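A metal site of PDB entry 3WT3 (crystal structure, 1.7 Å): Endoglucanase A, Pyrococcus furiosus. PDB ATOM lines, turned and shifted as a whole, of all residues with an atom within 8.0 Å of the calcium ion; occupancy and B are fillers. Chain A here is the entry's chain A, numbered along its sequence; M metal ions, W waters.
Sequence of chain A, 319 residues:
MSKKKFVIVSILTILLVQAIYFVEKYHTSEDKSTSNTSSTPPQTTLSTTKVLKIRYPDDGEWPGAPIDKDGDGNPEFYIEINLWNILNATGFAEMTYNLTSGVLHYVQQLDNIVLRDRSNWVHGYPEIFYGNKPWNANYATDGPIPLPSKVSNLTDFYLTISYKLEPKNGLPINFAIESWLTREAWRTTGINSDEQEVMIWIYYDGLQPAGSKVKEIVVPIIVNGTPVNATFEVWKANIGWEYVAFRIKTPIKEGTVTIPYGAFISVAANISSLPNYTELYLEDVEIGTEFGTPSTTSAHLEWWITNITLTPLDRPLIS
OD1 of Asn 136 is in hydrogen-bond range of N of Asn 138 (2.9 Å).
O of Thr 188 lies close to N of Asn 136 (3.4 Å).
The side-chain carboxylate (OE2) of Glu 80 is in hydrogen-bond range of the side-chain amide nitrogen (ND2) of Asn 136, at 2.9 Å.
OE1 of Glu 80 lies within salt-bridge range of NZ of Lys 133, 2.7 Å away.
The side-chain amide nitrogen of Asn 132 is in hydrogen-bond range of the backbone carbonyl oxygen of Arg 187 (2.9 Å).
The backbone NH (N) of Asn 132 is in hydrogen-bond range of the backbone carbonyl oxygen (O) of Glu 283, 2.9 Å away.
ND2 of Asn 132 sits at hydrogen-bond distance from O of Ala 185, 3.4 Å away.
ND2 of Asn 138 sits at hydrogen-bond distance from OE2 of Glu 80 (2.9 Å).
Residues that only touch the calcium ion: Ala 137 (3.6 Å).
Five residues have an atom within 4 Å of the calcium ion: Asn 132, Lys 133, Asn 136, Ala 137 and Asn 138.
The nearest printed residue that does not touch the calcium ion is Arg 187 (4.2 Å).
The calcium ion is bound by O of Asn 136 (2.3 Å), O of Lys 133 (2.3 Å), OD1 of Asn 132 (2.4 Å), O of Asn 138 (2.4 Å) and water W1 (2.4 Å).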
ATOM      1  N   GLU A  80      25.853 -23.735  32.580  1.00  0.00           N
ATOM      2  CA  GLU A  80      26.414 -24.849  31.758  1.00  0.00           C
ATOM      3  C   GLU A  80      27.539 -25.457  32.513  1.00  0.00           C
ATOM      4  O   GLU A  80      28.422 -24.786  33.053  1.00  0.00           O
ATOM      5  CB  GLU A  80      26.969 -24.319  30.389  1.00  0.00           C
ATOM      6  CG  GLU A  80      25.861 -23.719  29.501  1.00  0.00           C
ATOM      7  CD  GLU A  80      26.429 -23.280  28.116  1.00  0.00           C
ATOM      8  OE1 GLU A  80      27.626 -23.581  27.822  1.00  0.00           O
ATOM      9  OE2 GLU A  80      25.712 -22.581  27.430  1.00  0.00           O
ATOM     10  N   PHE A 129      25.943 -17.537  33.004  1.00  0.00           N
ATOM     11  CA  PHE A 129      26.168 -16.290  32.196  1.00  0.00           C
ATOM     12  C   PHE A 129      24.861 -15.541  31.966  1.00  0.00           C
ATOM     13  O   PHE A 129      23.734 -16.064  32.205  1.00  0.00           O
ATOM     14  CB  PHE A 129      26.830 -16.708  30.849  1.00  0.00           C
ATOM     15  CG  PHE A 129      25.904 -17.430  29.848  1.00  0.00           C
ATOM     16  CD1 PHE A 129      25.030 -16.701  29.036  1.00  0.00           C
ATOM     17  CD2 PHE A 129      25.996 -18.826  29.694  1.00  0.00           C
ATOM     18  CE1 PHE A 129      24.312 -17.376  28.064  1.00  0.00           C
ATOM     19  CE2 PHE A 129      25.224 -19.461  28.729  1.00  0.00           C
ATOM     20  CZ  PHE A 129      24.344 -18.762  27.945  1.00  0.00           C
ATOM     21  N   GLY A 131      23.259 -12.815  28.907  1.00  0.00           N
ATOM     22  CA  GLY A 131      23.491 -12.361  27.503  1.00  0.00           C
ATOM     23  C   GLY A 131      23.350 -13.483  26.566  1.00  0.00           C
ATOM     24  O   GLY A 131      22.735 -14.547  26.869  1.00  0.00           O
ATOM     25  N   ASN A 132      23.905 -13.293  25.373  1.00  0.00           N
ATOM     26  CA  ASN A 132      23.906 -14.334  24.398  1.00  0.00           C
ATOM     27  C   ASN A 132      25.276 -15.015  24.368  1.00  0.00           C
ATOM     28  O   ASN A 132      26.256 -14.363  24.001  1.00  0.00           O
ATOM     29  CB  ASN A 132      23.656 -13.777  22.958  1.00  0.00           C
ATOM     30  CG  ASN A 132      23.762 -14.869  21.936  1.00  0.00           C
ATOM     31  OD1 ASN A 132      23.262 -15.975  22.139  1.00  0.00           O
ATOM     32  ND2 ASN A 132      24.496 -14.624  20.870  1.00  0.00           N
ATOM     33  N   LYS A 133      25.352 -16.273  24.758  1.00  0.00           N
ATOM     34  CA  LYS A 133      26.608 -16.999  24.611  1.00  0.00           C
ATOM     35  C   LYS A 133      26.755 -17.385  23.099  1.00  0.00           C
ATOM     36  O   LYS A 133      25.907 -18.092  22.578  1.00  0.00           O
ATOM     37  CB  LYS A 133      26.683 -18.265  25.457  1.00  0.00           C
ATOM     38  CG  LYS A 133      27.999 -19.001  25.274  1.00  0.00           C
ATOM     39  CD  LYS A 133      28.132 -20.074  26.405  1.00  0.00           C
ATOM     40  CE  LYS A 133      29.417 -20.855  26.053  1.00  0.00           C
ATOM     41  NZ  LYS A 133      29.682 -21.995  27.042  1.00  0.00           N
ATOM     42  N   PRO A 134      27.854 -16.915  22.451  1.00  0.00           N
ATOM     43  CA  PRO A 134      27.881 -17.087  20.966  1.00  0.00           C
ATOM     44  C   PRO A 134      28.234 -18.460  20.470  1.00  0.00           C
ATOM     45  O   PRO A 134      28.163 -18.732  19.228  1.00  0.00           O
ATOM     46  CB  PRO A 134      28.956 -16.006  20.527  1.00  0.00           C
ATOM     47  CG  PRO A 134      29.940 -16.029  21.742  1.00  0.00           C
ATOM     48  CD  PRO A 134      28.976 -16.104  22.968  1.00  0.00           C
ATOM     49  N   TRP A 135      28.642 -19.378  21.360  1.00  0.00           N
ATOM     50  CA  TRP A 135      29.022 -20.737  20.913  1.00  0.00           C
ATOM     51  C   TRP A 135      27.859 -21.717  20.845  1.00  0.00           C
ATOM     52  O   TRP A 135      28.043 -22.842  20.322  1.00  0.00           O
ATOM     53  CB  TRP A 135      30.014 -21.265  21.991  1.00  0.00           C
ATOM     54  CG  TRP A 135      31.302 -20.568  21.956  1.00  0.00           C
ATOM     55  CD1 TRP A 135      31.735 -19.503  22.744  1.00  0.00           C
ATOM     56  CD2 TRP A 135      32.376 -20.853  21.049  1.00  0.00           C
ATOM     57  NE1 TRP A 135      33.009 -19.147  22.398  1.00  0.00           N
ATOM     58  CE2 TRP A 135      33.456 -19.981  21.375  1.00  0.00           C
ATOM     59  CE3 TRP A 135      32.536 -21.814  20.049  1.00  0.00           C
ATOM     60  CZ2 TRP A 135      34.698 -19.978  20.657  1.00  0.00           C
ATOM     61  CZ3 TRP A 135      33.753 -21.834  19.315  1.00  0.00           C
ATOM     62  CH2 TRP A 135      34.831 -20.913  19.623  1.00  0.00           C
ATOM     63  N   ASN A 136      26.694 -21.278  21.265  1.00  0.00           N
ATOM     64  CA  ASN A 136      25.507 -22.116  21.172  1.00  0.00           C
ATOM     65  C   ASN A 136      24.220 -21.330  21.110  1.00  0.00           C
ATOM     66  O   ASN A 136      24.234 -20.105  21.075  1.00  0.00           O
ATOM     67  CB  ASN A 136      25.518 -23.158  22.323  1.00  0.00           C
ATOM     68  CG  ASN A 136      25.545 -22.499  23.670  1.00  0.00           C
ATOM     69  OD1 ASN A 136      24.881 -21.455  23.852  1.00  0.00           O
ATOM     70  ND2 ASN A 136      26.383 -23.009  24.619  1.00  0.00           N
ATOM     71  N   ALA A 137      23.110 -22.083  21.152  1.00  0.00           N
ATOM     72  CA  ALA A 137      21.791 -21.432  21.071  1.00  0.00           C
ATOM     73  C   ALA A 137      21.241 -20.951  22.427  1.00  0.00           C
ATOM     74  O   ALA A 137      20.106 -20.596  22.551  1.00  0.00           O
ATOM     75  CB  ALA A 137      20.777 -22.369  20.394  1.00  0.00           C
ATOM     76  N   ASN A 138      22.109 -20.878  23.433  1.00  0.00           N
ATOM     77  CA  ASN A 138      21.635 -20.513  24.752  1.00  0.00           C
ATOM     78  C   ASN A 138      21.789 -19.050  25.002  1.00  0.00           C
ATOM     79  O   ASN A 138      22.754 -18.409  24.550  1.00  0.00           O
ATOM     80  CB  ASN A 138      22.431 -21.297  25.847  1.00  0.00           C
ATOM     81  CG  ASN A 138      22.319 -22.802  25.679  1.00  0.00           C
ATOM     82  OD1 ASN A 138      21.298 -23.322  25.141  1.00  0.00           O
ATOM     83  ND2 ASN A 138      23.339 -23.533  26.126  1.00  0.00           N
ATOM     84  N   TYR A 139      20.850 -18.504  25.766  1.00  0.00           N
ATOM     85  CA  TYR A 139      20.841 -17.093  26.103  1.00  0.00           C
ATOM     86  C   TYR A 139      20.021 -16.774  27.311  1.00  0.00           C
ATOM     87  O   TYR A 139      19.229 -17.559  27.725  1.00  0.00           O
ATOM     88  CB  TYR A 139      20.397 -16.203  24.905  1.00  0.00           C
ATOM     89  CG  TYR A 139      18.954 -16.444  24.504  1.00  0.00           C
ATOM     90  CD1 TYR A 139      17.973 -15.726  25.198  1.00  0.00           C
ATOM     91  CD2 TYR A 139      18.589 -17.439  23.538  1.00  0.00           C
ATOM     92  CE1 TYR A 139      16.612 -15.937  24.888  1.00  0.00           C
ATOM     93  CE2 TYR A 139      17.252 -17.645  23.228  1.00  0.00           C
ATOM     94  CZ  TYR A 139      16.279 -16.905  23.927  1.00  0.00           C
ATOM     95  OH  TYR A 139      14.923 -17.048  23.644  1.00  0.00           O
ATOM     96  N   ALA A 140      20.247 -15.597  27.847  1.00  0.00           N
ATOM     97  CA  ALA A 140      19.508 -15.118  29.035  1.00  0.00           C
ATOM     98  C   ALA A 140      19.572 -13.595  28.913  1.00  0.00           C
ATOM     99  O   ALA A 140      20.597 -12.969  29.113  1.00  0.00           O
ATOM    100  CB  ALA A 140      20.185 -15.586  30.353  1.00  0.00           C
ATOM    101  N   ALA A 185      25.169  -9.829  16.407  1.00  0.00           N
ATOM    102  CA  ALA A 185      24.653  -9.824  17.804  1.00  0.00           C
ATOM    103  C   ALA A 185      24.184 -11.160  18.242  1.00  0.00           C
ATOM    104  O   ALA A 185      24.350 -11.556  19.441  1.00  0.00           O
ATOM    105  CB  ALA A 185      23.521  -8.788  17.986  1.00  0.00           C
ATOM    106  N   TRP A 186      23.457 -11.873  17.357  1.00  0.00           N
ATOM    107  CA  TRP A 186      22.828 -13.113  17.762  1.00  0.00           C
ATOM    108  C   TRP A 186      23.564 -14.281  17.149  1.00  0.00           C
ATOM    109  O   TRP A 186      23.024 -15.206  16.608  1.00  0.00           O
ATOM    110  CB  TRP A 186      21.303 -13.074  17.455  1.00  0.00           C
ATOM    111  CG  TRP A 186      20.690 -12.239  18.529  1.00  0.00           C
ATOM    112  CD1 TRP A 186      20.371 -10.927  18.486  1.00  0.00           C
ATOM    113  CD2 TRP A 186      20.397 -12.706  19.844  1.00  0.00           C
ATOM    114  NE1 TRP A 186      19.917 -10.516  19.719  1.00  0.00           N
ATOM    115  CE2 TRP A 186      19.879 -11.604  20.566  1.00  0.00           C
ATOM    116  CE3 TRP A 186      20.424 -13.975  20.454  1.00  0.00           C
ATOM    117  CZ2 TRP A 186      19.473 -11.721  21.910  1.00  0.00           C
ATOM    118  CZ3 TRP A 186      19.976 -14.104  21.845  1.00  0.00           C
ATOM    119  CH2 TRP A 186      19.540 -12.981  22.514  1.00  0.00           C
ATOM    120  N   ARG A 187      24.891 -14.278  17.282  1.00  0.00           N
ATOM    121  CA  ARG A 187      25.687 -15.458  16.853  1.00  0.00           C
ATOM    122  C   ARG A 187      25.399 -16.700  17.683  1.00  0.00           C
ATOM    123  O   ARG A 187      25.283 -16.533  18.905  1.00  0.00           O
ATOM    124  CB  ARG A 187      27.132 -15.063  17.171  1.00  0.00           C
ATOM    125  CG  ARG A 187      28.162 -16.157  16.874  1.00  0.00           C
ATOM    126  CD  ARG A 187      28.314 -16.526  15.353  1.00  0.00           C
ATOM    127  NE  ARG A 187      28.638 -15.298  14.612  1.00  0.00           N
ATOM    128  CZ  ARG A 187      29.792 -14.619  14.634  1.00  0.00           C
ATOM    129  NH1 ARG A 187      30.827 -15.045  15.389  1.00  0.00           N
ATOM    130  NH2 ARG A 187      29.945 -13.513  13.922  1.00  0.00           N
ATOM    131  N   THR A 188      25.338 -17.931  17.102  1.00  0.00           N
ATOM    132  CA  THR A 188      25.165 -19.125  17.883  1.00  0.00           C
ATOM    133  C   THR A 188      26.134 -20.211  17.443  1.00  0.00           C
ATOM    134  O   THR A 188      26.028 -21.315  17.939  1.00  0.00           O
ATOM    135  CB  THR A 188      23.739 -19.738  17.745  1.00  0.00           C
ATOM    136  OG1 THR A 188      23.544 -19.986  16.308  1.00  0.00           O
ATOM    137  CG2 THR A 188      22.709 -18.721  18.173  1.00  0.00           C
ATOM    138  N   THR A 189      27.045 -19.930  16.488  1.00  0.00           N
ATOM    139  CA  THR A 189      27.873 -20.968  15.895  1.00  0.00           C
ATOM    140  C   THR A 189      29.377 -20.777  16.096  1.00  0.00           C
ATOM    141  O   THR A 189      30.206 -21.438  15.413  1.00  0.00           O
ATOM    142  CB  THR A 189      27.557 -21.134  14.366  1.00  0.00           C
ATOM    143  OG1 THR A 189      27.671 -19.859  13.779  1.00  0.00           O
ATOM    144  CG2 THR A 189      26.139 -21.636  14.229  1.00  0.00           C
ATOM    145  N   GLU A 283      28.562  -9.552  23.670  1.00  0.00           N
ATOM    146  CA  GLU A 283      27.562 -10.546  23.572  1.00  0.00           C
ATOM    147  C   GLU A 283      26.943 -10.869  24.958  1.00  0.00           C
ATOM    148  O   GLU A 283      25.747 -11.130  25.037  1.00  0.00           O
ATOM    149  CB  GLU A 283      28.208 -11.859  23.085  1.00  0.00           C
ATOM    150  CG  GLU A 283      28.566 -11.681  21.574  1.00  0.00           C
ATOM    151  CD  GLU A 283      27.328 -11.888  20.771  1.00  0.00           C
ATOM    152  OE1 GLU A 283      27.106 -12.997  20.263  1.00  0.00           O
ATOM    153  OE2 GLU A 283      26.602 -10.869  20.612  1.00  0.00           O
ATOM    154  N   ASP A 284      27.852 -10.905  25.924  1.00  0.00           N
ATOM    155  CA  ASP A 284      27.460 -11.569  27.217  1.00  0.00           C
ATOM    156  C   ASP A 284      28.473 -11.296  28.303  1.00  0.00           C
ATOM    157  O   ASP A 284      29.501 -10.653  28.044  1.00  0.00           O
ATOM    158  CB  ASP A 284      27.318 -13.122  26.950  1.00  0.00           C
ATOM    159  CG  ASP A 284      28.642 -13.866  26.629  1.00  0.00           C
ATOM    160  OD1 ASP A 284      29.708 -13.264  26.352  1.00  0.00           O
ATOM    161  OD2 ASP A 284      28.506 -15.168  26.671  1.00  0.00           O
HETATM  162 CA    CA M   1      23.609 -18.307  22.345  1.00  0.00          CA
HETATM  163  O   HOH W   1      21.390 -17.989  21.389  1.00  0.00           O
